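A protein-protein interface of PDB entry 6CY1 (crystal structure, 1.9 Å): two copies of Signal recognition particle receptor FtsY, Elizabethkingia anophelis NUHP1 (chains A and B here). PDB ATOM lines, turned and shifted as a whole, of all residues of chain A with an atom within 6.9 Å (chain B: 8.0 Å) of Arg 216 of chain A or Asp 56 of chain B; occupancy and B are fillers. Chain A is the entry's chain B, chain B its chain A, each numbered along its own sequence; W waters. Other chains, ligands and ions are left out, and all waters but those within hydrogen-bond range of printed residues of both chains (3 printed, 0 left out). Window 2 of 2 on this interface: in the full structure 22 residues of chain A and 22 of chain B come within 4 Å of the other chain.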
ATOM      1  N   GLY A 130      18.218 -12.963 -10.222  1.00  0.00           N
ATOM      2  CA  GLY A 130      17.918 -11.558 -10.440  1.00  0.00           C
ATOM      3  C   GLY A 130      16.578 -11.357 -11.130  1.00  0.00           C
ATOM      4  O   GLY A 130      15.933 -12.331 -11.536  1.00  0.00           O
ATOM      5  N   VAL A 131      16.140 -10.106 -11.259  1.00  0.00           N
ATOM      6  CA  VAL A 131      14.828  -9.803 -11.834  1.00  0.00           C
ATOM      7  C   VAL A 131      14.882  -9.692 -13.356  1.00  0.00           C
ATOM      8  O   VAL A 131      15.967  -9.660 -13.950  1.00  0.00           O
ATOM      9  CB  VAL A 131      14.257  -8.516 -11.220  1.00  0.00           C
ATOM     10  CG1 VAL A 131      14.238  -8.630  -9.698  1.00  0.00           C
ATOM     11  CG2 VAL A 131      15.076  -7.321 -11.666  1.00  0.00           C
ATOM     12  N   ASN A 132      13.709  -9.647 -13.993  1.00  0.00           N
ATOM     13  CA  ASN A 132      13.639  -9.473 -15.439  1.00  0.00           C
ATOM     14  C   ASN A 132      14.174  -8.093 -15.819  1.00  0.00           C
ATOM     15  O   ASN A 132      13.938  -7.104 -15.117  1.00  0.00           O
ATOM     16  CB  ASN A 132      12.187  -9.577 -15.937  1.00  0.00           C
ATOM     17  CG  ASN A 132      11.551 -10.945 -15.706  1.00  0.00           C
ATOM     18  OD1 ASN A 132      12.188 -11.877 -15.223  1.00  0.00           O
ATOM     19  ND2 ASN A 132      10.279 -11.068 -16.087  1.00  0.00           N
ATOM     20  N   LYS A 136      20.324 -10.601 -17.229  1.00  0.00           N
ATOM     21  CA  LYS A 136      20.733 -11.923 -16.764  1.00  0.00           C
ATOM     22  C   LYS A 136      21.151 -12.831 -17.913  1.00  0.00           C
ATOM     23  O   LYS A 136      22.199 -13.477 -17.848  1.00  0.00           O
ATOM     24  CB  LYS A 136      19.605 -12.585 -15.980  1.00  0.00           C
ATOM     25  CG  LYS A 136      19.462 -12.116 -14.558  1.00  0.00           C
ATOM     26  CD  LYS A 136      18.600 -13.087 -13.755  1.00  0.00           C
ATOM     27  CE  LYS A 136      17.251 -13.310 -14.412  1.00  0.00           C
ATOM     28  NZ  LYS A 136      16.346 -14.096 -13.526  1.00  0.00           N
ATOM     29  N   ASP A 160      14.380 -20.720 -16.066  1.00  0.00           N
ATOM     30  CA  ASP A 160      13.270 -19.756 -16.046  1.00  0.00           C
ATOM     31  C   ASP A 160      12.250 -20.227 -17.077  1.00  0.00           C
ATOM     32  O   ASP A 160      12.221 -19.783 -18.226  1.00  0.00           O
ATOM     33  CB  ASP A 160      13.734 -18.330 -16.319  1.00  0.00           C
ATOM     34  CG  ASP A 160      12.600 -17.306 -16.151  1.00  0.00           C
ATOM     35  OD1 ASP A 160      11.457 -17.719 -15.866  1.00  0.00           O
ATOM     36  OD2 ASP A 160      12.854 -16.091 -16.297  1.00  0.00           O
ATOM     37  N   PHE A 162       8.941 -20.163 -17.374  1.00  0.00           N
ATOM     38  CA  PHE A 162       7.684 -19.505 -17.698  1.00  0.00           C
ATOM     39  C   PHE A 162       7.843 -18.260 -18.555  1.00  0.00           C
ATOM     40  O   PHE A 162       6.836 -17.710 -19.002  1.00  0.00           O
ATOM     41  CB  PHE A 162       6.930 -19.158 -16.409  1.00  0.00           C
ATOM     42  CG  PHE A 162       6.302 -20.354 -15.746  1.00  0.00           C
ATOM     43  CD1 PHE A 162       4.984 -20.702 -16.017  1.00  0.00           C
ATOM     44  CD2 PHE A 162       7.036 -21.151 -14.877  1.00  0.00           C
ATOM     45  CE1 PHE A 162       4.403 -21.811 -15.422  1.00  0.00           C
ATOM     46  CE2 PHE A 162       6.460 -22.260 -14.275  1.00  0.00           C
ATOM     47  CZ  PHE A 162       5.143 -22.593 -14.550  1.00  0.00           C
ATOM     48  N   ARG A 163       9.063 -17.817 -18.819  1.00  0.00           N
ATOM     49  CA  ARG A 163       9.305 -16.603 -19.593  1.00  0.00           C
ATOM     50  C   ARG A 163       9.933 -16.988 -20.929  1.00  0.00           C
ATOM     51  O   ARG A 163      11.118 -17.337 -20.989  1.00  0.00           O
ATOM     52  CB  ARG A 163      10.190 -15.635 -18.813  1.00  0.00           C
ATOM     53  CG  ARG A 163      10.385 -14.301 -19.499  1.00  0.00           C
ATOM     54  CD  ARG A 163      10.796 -13.239 -18.496  1.00  0.00           C
ATOM     55  NE  ARG A 163      12.189 -13.357 -18.094  1.00  0.00           N
ATOM     56  CZ  ARG A 163      13.132 -12.467 -18.397  1.00  0.00           C
ATOM     57  NH1 ARG A 163      12.827 -11.386 -19.107  1.00  0.00           N
ATOM     58  NH2 ARG A 163      14.378 -12.660 -17.984  1.00  0.00           N
ATOM     59  N   ALA A 214      14.169 -17.896 -12.533  1.00  0.00           N
ATOM     60  CA  ALA A 214      13.184 -16.822 -12.531  1.00  0.00           C
ATOM     61  C   ALA A 214      13.425 -15.906 -11.339  1.00  0.00           C
ATOM     62  O   ALA A 214      13.916 -16.332 -10.293  1.00  0.00           O
ATOM     63  CB  ALA A 214      11.761 -17.383 -12.494  1.00  0.00           C
ATOM     64  N   GLY A 215      13.094 -14.627 -11.508  1.00  0.00           N
ATOM     65  CA  GLY A 215      13.289 -13.661 -10.439  1.00  0.00           C
ATOM     66  C   GLY A 215      12.229 -12.574 -10.408  1.00  0.00           C
ATOM     67  O   GLY A 215      11.800 -12.103 -11.462  1.00  0.00           O
ATOM     68  N   ARG A 216      11.828 -12.154  -9.208  1.00  0.00           N
ATOM     69  CA  ARG A 216      10.808 -11.130  -9.007  1.00  0.00           C
ATOM     70  C   ARG A 216      10.743 -10.786  -7.525  1.00  0.00           C
ATOM     71  O   ARG A 216      10.813 -11.681  -6.682  1.00  0.00           O
ATOM     72  CB  ARG A 216       9.436 -11.608  -9.496  1.00  0.00           C
ATOM     73  CG  ARG A 216       8.887 -12.790  -8.711  1.00  0.00           C
ATOM     74  CD  ARG A 216       7.668 -13.396  -9.385  1.00  0.00           C
ATOM     75  NE  ARG A 216       7.982 -13.822 -10.745  1.00  0.00           N
ATOM     76  CZ  ARG A 216       8.714 -14.892 -11.044  1.00  0.00           C
ATOM     77  NH1 ARG A 216       8.950 -15.201 -12.313  1.00  0.00           N
ATOM     78  NH2 ARG A 216       9.215 -15.652 -10.075  1.00  0.00           N
ATOM     79  N   LEU A 217      10.650  -9.490  -7.209  1.00  0.00           N
ATOM     80  CA  LEU A 217      10.601  -9.108  -5.799  1.00  0.00           C
ATOM     81  C   LEU A 217       9.211  -9.332  -5.199  1.00  0.00           C
ATOM     82  O   LEU A 217       9.087  -9.659  -4.015  1.00  0.00           O
ATOM     83  CB  LEU A 217      11.010  -7.641  -5.641  1.00  0.00           C
ATOM     84  N   HIS A 218       8.154  -9.124  -5.977  1.00  0.00           N
ATOM     85  CA  HIS A 218       6.824  -9.398  -5.462  1.00  0.00           C
ATOM     86  C   HIS A 218       6.642 -10.907  -5.408  1.00  0.00           C
ATOM     87  O   HIS A 218       7.275 -11.651  -6.160  1.00  0.00           O
ATOM     88  CB  HIS A 218       5.758  -8.707  -6.312  1.00  0.00           C
ATOM     89  CG  HIS A 218       5.392  -9.439  -7.561  1.00  0.00           C
ATOM     90  ND1 HIS A 218       6.198  -9.460  -8.678  1.00  0.00           N
ATOM     91  CD2 HIS A 218       4.273 -10.130  -7.888  1.00  0.00           C
ATOM     92  CE1 HIS A 218       5.602 -10.150  -9.634  1.00  0.00           C
ATOM     93  NE2 HIS A 218       4.431 -10.565  -9.183  1.00  0.00           N
ATOM     94  N   ASN A 219       5.791 -11.365  -4.503  1.00  0.00           N
ATOM     95  CA  ASN A 219       5.694 -12.796  -4.204  1.00  0.00           C
ATOM     96  C   ASN A 219       7.082 -13.371  -3.900  1.00  0.00           C
ATOM     97  O   ASN A 219       7.561 -14.338  -4.515  1.00  0.00           O
ATOM     98  CB  ASN A 219       5.017 -13.555  -5.351  1.00  0.00           C
ATOM     99  N   LYS A 220       7.730 -12.753  -2.912  1.00  0.00           N
ATOM    100  CA  LYS A 220       9.082 -13.166  -2.552  1.00  0.00           C
ATOM    101  C   LYS A 220       9.097 -14.563  -1.940  1.00  0.00           C
ATOM    102  O   LYS A 220      10.040 -15.323  -2.160  1.00  0.00           O
ATOM    103  CB  LYS A 220       9.700 -12.158  -1.588  1.00  0.00           C
ATOM    104  N   ASN A 222       7.347 -17.231  -2.646  1.00  0.00           N
ATOM    105  CA  ASN A 222       7.388 -18.256  -3.675  1.00  0.00           C
ATOM    106  C   ASN A 222       8.733 -18.261  -4.372  1.00  0.00           C
ATOM    107  O   ASN A 222       9.248 -19.328  -4.733  1.00  0.00           O
ATOM    108  CB  ASN A 222       6.239 -18.043  -4.665  1.00  0.00           C
ATOM    109  CG  ASN A 222       4.873 -18.018  -3.982  1.00  0.00           C
ATOM    110  OD1 ASN A 222       4.038 -17.162  -4.278  1.00  0.00           O
ATOM    111  ND2 ASN A 222       4.645 -18.952  -3.056  1.00  0.00           N
ATOM    112  N   LEU A 223       9.355 -17.090  -4.505  1.00  0.00           N
ATOM    113  CA  LEU A 223      10.682 -17.030  -5.113  1.00  0.00           C
ATOM    114  C   LEU A 223      11.720 -17.761  -4.268  1.00  0.00           C
ATOM    115  O   LEU A 223      12.510 -18.552  -4.795  1.00  0.00           O
ATOM    116  CB  LEU A 223      11.103 -15.577  -5.304  1.00  0.00           C
ATOM    117  CG  LEU A 223      12.505 -15.458  -5.898  1.00  0.00           C
ATOM    118  CD1 LEU A 223      12.516 -16.033  -7.305  1.00  0.00           C
ATOM    119  CD2 LEU A 223      12.977 -14.015  -5.878  1.00  0.00           C
ATOM    120  N   GLU A 226      11.283 -21.489  -4.515  1.00  0.00           N
ATOM    121  CA  GLU A 226      11.720 -22.038  -5.795  1.00  0.00           C
ATOM    122  C   GLU A 226      13.236 -22.133  -5.862  1.00  0.00           C
ATOM    123  O   GLU A 226      13.783 -23.141  -6.329  1.00  0.00           O
ATOM    124  CB  GLU A 226      11.178 -21.187  -6.947  1.00  0.00           C
ATOM    125  CG  GLU A 226      11.377 -21.850  -8.321  1.00  0.00           C
ATOM    126  CD  GLU A 226      10.906 -20.985  -9.479  1.00  0.00           C
ATOM    127  OE1 GLU A 226      11.667 -20.101  -9.925  1.00  0.00           O
ATOM    128  OE2 GLU A 226       9.763 -21.195  -9.940  1.00  0.00           O
ATOM    129  N   PHE A 264      17.236  -9.240  -2.345  1.00  0.00           N
ATOM    130  CA  PHE A 264      17.577 -10.581  -2.813  1.00  0.00           C
ATOM    131  C   PHE A 264      18.537 -11.283  -1.864  1.00  0.00           C
ATOM    132  O   PHE A 264      18.365 -12.472  -1.572  1.00  0.00           O
ATOM    133  CB  PHE A 264      18.204 -10.492  -4.204  1.00  0.00           C
ATOM    134  CG  PHE A 264      17.485 -11.269  -5.257  1.00  0.00           C
ATOM    135  CD1 PHE A 264      17.674 -12.637  -5.375  1.00  0.00           C
ATOM    136  CD2 PHE A 264      16.635 -10.634  -6.146  1.00  0.00           C
ATOM    137  CE1 PHE A 264      17.009 -13.363  -6.351  1.00  0.00           C
ATOM    138  CE2 PHE A 264      15.968 -11.354  -7.124  1.00  0.00           C
ATOM    139  CZ  PHE A 264      16.158 -12.718  -7.225  1.00  0.00           C
ATOM    140  N   ALA B  43       7.295  -3.514 -21.489  1.00  0.00           N
ATOM    141  CA  ALA B  43       6.640  -4.539 -20.688  1.00  0.00           C
ATOM    142  C   ALA B  43       5.413  -5.127 -21.368  1.00  0.00           C
ATOM    143  O   ALA B  43       4.941  -6.189 -20.947  1.00  0.00           O
ATOM    144  CB  ALA B  43       6.241  -3.966 -19.328  1.00  0.00           C
ATOM    145  N   VAL B  50      -2.954  -8.268 -19.313  1.00  0.00           N
ATOM    146  CA  VAL B  50      -2.027  -8.129 -18.195  1.00  0.00           C
ATOM    147  C   VAL B  50      -1.897  -9.503 -17.541  1.00  0.00           C
ATOM    148  O   VAL B  50      -2.832  -9.984 -16.896  1.00  0.00           O
ATOM    149  CB  VAL B  50      -2.512  -7.069 -17.196  1.00  0.00           C
ATOM    150  CG1 VAL B  50      -1.556  -6.946 -16.010  1.00  0.00           C
ATOM    151  CG2 VAL B  50      -2.661  -5.727 -17.884  1.00  0.00           C
ATOM    152  N   ASP B  51      -0.757 -10.160 -17.740  1.00  0.00           N
ATOM    153  CA  ASP B  51      -0.509 -11.464 -17.138  1.00  0.00           C
ATOM    154  C   ASP B  51       0.685 -11.372 -16.196  1.00  0.00           C
ATOM    155  O   ASP B  51       1.219 -10.289 -15.942  1.00  0.00           O
ATOM    156  CB  ASP B  51      -0.291 -12.544 -18.206  1.00  0.00           C
ATOM    157  CG  ASP B  51       0.902 -12.268 -19.118  1.00  0.00           C
ATOM    158  OD1 ASP B  51       1.739 -11.392 -18.825  1.00  0.00           O
ATOM    159  OD2 ASP B  51       1.012 -12.959 -20.149  1.00  0.00           O
ATOM    160  N   ASP B  52       1.116 -12.535 -15.696  1.00  0.00           N
ATOM    161  CA  ASP B  52       2.196 -12.565 -14.714  1.00  0.00           C
ATOM    162  C   ASP B  52       3.475 -11.967 -15.280  1.00  0.00           C
ATOM    163  O   ASP B  52       4.199 -11.255 -14.576  1.00  0.00           O
ATOM    164  CB  ASP B  52       2.442 -13.998 -14.240  1.00  0.00           C
ATOM    165  CG  ASP B  52       1.297 -14.540 -13.410  1.00  0.00           C
ATOM    166  OD1 ASP B  52       0.517 -13.722 -12.878  1.00  0.00           O
ATOM    167  OD2 ASP B  52       1.181 -15.777 -13.282  1.00  0.00           O
ATOM    168  N   GLU B  53       3.769 -12.243 -16.548  1.00  0.00           N
ATOM    169  CA  GLU B  53       4.983 -11.695 -17.140  1.00  0.00           C
ATOM    170  C   GLU B  53       4.905 -10.179 -17.258  1.00  0.00           C
ATOM    171  O   GLU B  53       5.906  -9.489 -17.046  1.00  0.00           O
ATOM    172  CB  GLU B  53       5.250 -12.325 -18.507  1.00  0.00           C
ATOM    173  CG  GLU B  53       6.596 -11.915 -19.077  1.00  0.00           C
ATOM    174  CD  GLU B  53       6.925 -12.615 -20.377  1.00  0.00           C
ATOM    175  OE1 GLU B  53       6.324 -13.680 -20.646  1.00  0.00           O
ATOM    176  OE2 GLU B  53       7.814 -12.115 -21.105  1.00  0.00           O
ATOM    177  N   VAL B  54       3.730  -9.639 -17.599  1.00  0.00           N
ATOM    178  CA  VAL B  54       3.588  -8.185 -17.643  1.00  0.00           C
ATOM    179  C   VAL B  54       3.860  -7.591 -16.273  1.00  0.00           C
ATOM    180  O   VAL B  54       4.551  -6.575 -16.138  1.00  0.00           O
ATOM    181  CB  VAL B  54       2.182  -7.790 -18.137  1.00  0.00           C
ATOM    182  CG1 VAL B  54       1.958  -6.290 -17.967  1.00  0.00           C
ATOM    183  CG2 VAL B  54       1.995  -8.200 -19.578  1.00  0.00           C
ATOM    184  N   LEU B  55       3.329  -8.225 -15.231  1.00  0.00           N
ATOM    185  CA  LEU B  55       3.536  -7.683 -13.895  1.00  0.00           C
ATOM    186  C   LEU B  55       5.001  -7.793 -13.481  1.00  0.00           C
ATOM    187  O   LEU B  55       5.539  -6.875 -12.854  1.00  0.00           O
ATOM    188  CB  LEU B  55       2.611  -8.391 -12.913  1.00  0.00           C
ATOM    189  CG  LEU B  55       1.127  -8.094 -13.205  1.00  0.00           C
ATOM    190  CD1 LEU B  55       0.256  -8.742 -12.143  1.00  0.00           C
ATOM    191  CD2 LEU B  55       0.848  -6.611 -13.273  1.00  0.00           C
ATOM    192  N   ASP B  56       5.670  -8.897 -13.829  1.00  0.00           N
ATOM    193  CA  ASP B  56       7.105  -8.996 -13.550  1.00  0.00           C
ATOM    194  C   ASP B  56       7.874  -7.859 -14.210  1.00  0.00           C
ATOM    195  O   ASP B  56       8.724  -7.209 -13.582  1.00  0.00           O
ATOM    196  CB  ASP B  56       7.643 -10.342 -14.041  1.00  0.00           C
ATOM    197  CG  ASP B  56       7.147 -11.499 -13.208  1.00  0.00           C
ATOM    198  OD1 ASP B  56       6.530 -11.257 -12.153  1.00  0.00           O
ATOM    199  OD2 ASP B  56       7.375 -12.656 -13.599  1.00  0.00           O
ATOM    200  N   ASP B  57       7.580  -7.598 -15.484  1.00  0.00           N
ATOM    201  CA  ASP B  57       8.273  -6.525 -16.193  1.00  0.00           C
ATOM    202  C   ASP B  57       7.922  -5.166 -15.604  1.00  0.00           C
ATOM    203  O   ASP B  57       8.780  -4.279 -15.502  1.00  0.00           O
ATOM    204  CB  ASP B  57       7.925  -6.573 -17.680  1.00  0.00           C
ATOM    205  CG  ASP B  57       8.527  -7.784 -18.391  1.00  0.00           C
ATOM    206  OD1 ASP B  57       9.513  -8.363 -17.888  1.00  0.00           O
ATOM    207  OD2 ASP B  57       8.007  -8.163 -19.458  1.00  0.00           O
ATOM    208  N   LEU B  58       6.666  -4.988 -15.205  1.00  0.00           N
ATOM    209  CA  LEU B  58       6.263  -3.721 -14.607  1.00  0.00           C
ATOM    210  C   LEU B  58       6.974  -3.492 -13.288  1.00  0.00           C
ATOM    211  O   LEU B  58       7.301  -2.352 -12.947  1.00  0.00           O
ATOM    212  CB  LEU B  58       4.741  -3.697 -14.426  1.00  0.00           C
ATOM    213  CG  LEU B  58       4.094  -2.452 -13.818  1.00  0.00           C
ATOM    214  CD1 LEU B  58       4.238  -1.284 -14.775  1.00  0.00           C
ATOM    215  CD2 LEU B  58       2.621  -2.739 -13.546  1.00  0.00           C
ATOM    216  N   GLU B  59       7.226  -4.564 -12.539  1.00  0.00           N
ATOM    217  CA  GLU B  59       7.970  -4.439 -11.295  1.00  0.00           C
ATOM    218  C   GLU B  59       9.348  -3.823 -11.532  1.00  0.00           C
ATOM    219  O   GLU B  59       9.729  -2.854 -10.865  1.00  0.00           O
ATOM    220  CB  GLU B  59       8.115  -5.816 -10.656  1.00  0.00           C
ATOM    221  CG  GLU B  59       8.812  -5.792  -9.337  1.00  0.00           C
ATOM    222  CD  GLU B  59       8.809  -7.148  -8.675  1.00  0.00           C
ATOM    223  OE1 GLU B  59       9.173  -8.139  -9.341  1.00  0.00           O
ATOM    224  OE2 GLU B  59       8.382  -7.227  -7.503  1.00  0.00           O
ATOM    225  N   GLU B  60      10.106  -4.355 -12.495  1.00  0.00           N
ATOM    226  CA  GLU B  60      11.424  -3.775 -12.760  1.00  0.00           C
ATOM    227  C   GLU B  60      11.319  -2.356 -13.303  1.00  0.00           C
ATOM    228  O   GLU B  60      12.199  -1.528 -13.039  1.00  0.00           O
ATOM    229  CB  GLU B  60      12.235  -4.655 -13.713  1.00  0.00           C
ATOM    230  CG  GLU B  60      13.658  -4.113 -13.990  1.00  0.00           C
ATOM    231  CD  GLU B  60      14.421  -3.610 -12.731  1.00  0.00           C
ATOM    232  OE1 GLU B  60      14.190  -4.105 -11.604  1.00  0.00           O
ATOM    233  OE2 GLU B  60      15.276  -2.708 -12.876  1.00  0.00           O
ATOM    234  N   VAL B  61      10.270  -2.059 -14.074  1.00  0.00           N
ATOM    235  CA  VAL B  61      10.090  -0.700 -14.585  1.00  0.00           C
ATOM    236  C   VAL B  61       9.888   0.278 -13.441  1.00  0.00           C
ATOM    237  O   VAL B  61      10.466   1.376 -13.424  1.00  0.00           O
ATOM    238  CB  VAL B  61       8.904  -0.650 -15.565  1.00  0.00           C
ATOM    239  CG1 VAL B  61       8.495   0.794 -15.799  1.00  0.00           C
ATOM    240  CG2 VAL B  61       9.276  -1.328 -16.878  1.00  0.00           C
ATOM    241  N   LEU B  62       9.054  -0.094 -12.473  1.00  0.00           N
ATOM    242  CA  LEU B  62       8.826   0.775 -11.321  1.00  0.00           C
ATOM    243  C   LEU B  62      10.094   0.925 -10.491  1.00  0.00           C
ATOM    244  O   LEU B  62      10.391   2.022  -9.993  1.00  0.00           O
ATOM    245  CB  LEU B  62       7.677   0.221 -10.464  1.00  0.00           C
ATOM    246  CG  LEU B  62       6.302   0.377 -11.140  1.00  0.00           C
ATOM    247  CD1 LEU B  62       5.266  -0.524 -10.463  1.00  0.00           C
ATOM    248  CD2 LEU B  62       5.829   1.832 -11.106  1.00  0.00           C
ATOM    249  N   ILE B  63      10.829  -0.174 -10.289  1.00  0.00           N
ATOM    250  CA  ILE B  63      12.104  -0.084  -9.577  1.00  0.00           C
ATOM    251  C   ILE B  63      13.048   0.850 -10.312  1.00  0.00           C
ATOM    252  O   ILE B  63      13.696   1.713  -9.703  1.00  0.00           O
ATOM    253  CB  ILE B  63      12.739  -1.470  -9.375  1.00  0.00           C
ATOM    254  CG1 ILE B  63      11.847  -2.331  -8.497  1.00  0.00           C
ATOM    255  CG2 ILE B  63      14.126  -1.315  -8.733  1.00  0.00           C
ATOM    256  CD1 ILE B  63      11.628  -1.750  -7.149  1.00  0.00           C
ATOM    257  N   THR B  72       6.766  -0.543  -4.783  1.00  0.00           N
ATOM    258  CA  THR B  72       6.545  -1.265  -6.040  1.00  0.00           C
ATOM    259  C   THR B  72       5.815  -2.578  -5.808  1.00  0.00           C
ATOM    260  O   THR B  72       4.892  -2.926  -6.559  1.00  0.00           O
ATOM    261  CB  THR B  72       7.889  -1.533  -6.725  1.00  0.00           C
ATOM    262  OG1 THR B  72       8.440  -0.295  -7.165  1.00  0.00           O
ATOM    263  CG2 THR B  72       7.726  -2.474  -7.927  1.00  0.00           C
ATOM    264  N   VAL B  73       6.207  -3.321  -4.765  1.00  0.00           N
ATOM    265  CA  VAL B  73       5.547  -4.595  -4.454  1.00  0.00           C
ATOM    266  C   VAL B  73       4.074  -4.360  -4.116  1.00  0.00           C
ATOM    267  O   VAL B  73       3.190  -5.117  -4.543  1.00  0.00           O
ATOM    268  CB  VAL B  73       6.303  -5.320  -3.322  1.00  0.00           C
ATOM    269  CG1 VAL B  73       5.462  -6.443  -2.722  1.00  0.00           C
ATOM    270  CG2 VAL B  73       7.650  -5.863  -3.850  1.00  0.00           C
ATOM    271  N   ILE B  76       2.113  -3.695  -7.346  1.00  0.00           N
ATOM    272  CA  ILE B  76       1.875  -4.924  -8.094  1.00  0.00           C
ATOM    273  C   ILE B  76       0.759  -5.726  -7.445  1.00  0.00           C
ATOM    274  O   ILE B  76      -0.102  -6.286  -8.132  1.00  0.00           O
ATOM    275  CB  ILE B  76       3.174  -5.753  -8.186  1.00  0.00           C
ATOM    276  CG1 ILE B  76       4.251  -4.972  -8.931  1.00  0.00           C
ATOM    277  CG2 ILE B  76       2.923  -7.047  -8.935  1.00  0.00           C
ATOM    278  CD1 ILE B  76       3.930  -4.710 -10.378  1.00  0.00           C
ATOM    279  N   GLU B  80      -2.657  -6.977  -9.102  1.00  0.00           N
ATOM    280  CA  GLU B  80      -3.104  -8.373  -9.123  1.00  0.00           C
ATOM    281  C   GLU B  80      -4.529  -8.502  -8.588  1.00  0.00           C
ATOM    282  O   GLU B  80      -5.370  -9.183  -9.191  1.00  0.00           O
ATOM    283  CB  GLU B  80      -2.163  -9.253  -8.304  1.00  0.00           C
ATOM    284  CG  GLU B  80      -0.751  -9.344  -8.841  1.00  0.00           C
ATOM    285  CD  GLU B  80       0.139 -10.271  -8.022  1.00  0.00           C
ATOM    286  OE1 GLU B  80      -0.127 -10.454  -6.818  1.00  0.00           O
ATOM    287  OE2 GLU B  80       1.112 -10.814  -8.590  1.00  0.00           O
HETATM  288  O   HOH W   1       9.743 -10.564 -19.601  1.00  0.00           O
HETATM  289  O   HOH W   2       8.517 -13.228 -15.989  1.00  0.00           O
HETATM  290  O   HOH W   3       3.848 -11.641 -11.813  1.00  0.00           O
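Water W2 lies within hydrogen-bond range of OD2 of Asp 56 of chain B (2.7 Å) and ND2 of Asn 132 of chain A (2.8 Å).
Water W3 lies within hydrogen-bond range of OD1 of Asp 56 of chain B, O of Asp 52 of chain B and NE2 of His 218 of chain A.
Water W1 lies within hydrogen-bond range of the side-chain carboxylate (OD1) of Asp 57 of chain B (2.8 Å), the side-chain carboxylate (OE2) of Glu 53 of chain B (2.9 Å) and the guanidinium group (NH1) of Arg 163 of chain A (3.2 Å).
No position is printed for both chains.
Of the 19 printed residues of chain B, 8 touch a printed residue of chain A.
Among the printed residues, 13 pairs touch across the chains.
Among the printed residues, Asp or Glu carboxylates within 4 Å of a Lys or Arg side-chain nitrogen of the other chain: Arg 216 of chain A with Asp 56 of chain B.
Arg 216 of chain A touches two residues of chain B.
Asp 56 of chain B touches just these residues of chain A: Asn 132, Arg 216 and His 218.
No residue of chain B comes within 4 Å of Gly 215 of chain A.
Printed residues of chain A within 4 Å of Glu 80 of chain B: His 218 (3.3 Å).
Of the printed residues of chain B, His 218 of chain A touches Asp 56 (2.9 Å), Glu 59 (2.4 Å), Val 73 (3.9 Å), Ile 76 (3.5 Å) and Glu 80 (3.3 Å).
Of the printed residues of chain B, Val 131 of chain A touches Glu 60.
Printed residues of chain A within 4 Å of Glu 53 of chain B: Arg 163 (3.7 Å).
Printed residues of chain A within 4 Å of Glu 60 of chain B: Val 131 and Asn 132.
Lys 220 of chain A touches none of the printed residues of chain B.
Asn 219 of chain A touches none of the printed residues of chain B.
OD1 of Asp 51 of chain B lies within hydrogen-bond range of N of Glu 53 of chain B.
OD1 of Asn 132 of chain A sits at hydrogen-bond distance from NE of Arg 163 of chain A.
OD2 of Asp 160 of chain A is in salt-bridge range of NE of Arg 163 of chain A (3.3 Å).
The side-chain carboxylate (OD2) of Asp 56 of chain B lies within salt-bridge range of the guanidinium group (NE) of Arg 216 of chain A, at 3.1 Å.
The side-chain carboxylate of Asp 57 of chain B sits at hydrogen-bond distance from the side-chain amide nitrogen of Asn 132 of chain A.
N of Leu 217 of chain A sits at hydrogen-bond distance from OE1 of Glu 59 of chain B (2.9 Å).
OE2 of Glu 59 of chain B lies within hydrogen-bond range of N of His 218 of chain A (2.4 Å).
OE2 of Glu 80 of chain B lies close to NE2 of His 218 of chain A, 3.4 Å away.
Among the printed residues, merely in contact across the chains: Val 131 of chain A with Glu 60 of chain B (3.3 Å), Asn 132 of chain A with Asp 56 of chain B (3.4 Å), Asn 132 of chain A with Glu 60 of chain B (3.2 Å), Arg 163 of chain A with Glu 53 of chain B (3.7 Å), Arg 216 of chain A with Glu 59 of chain B (3.4 Å), His 218 of chain A with Asp 56 of chain B (2.9 Å), His 218 of chain A with Val 73 of chain B (3.9 Å) and His 218 of chain A with Ile 76 of chain B (3.5 Å).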
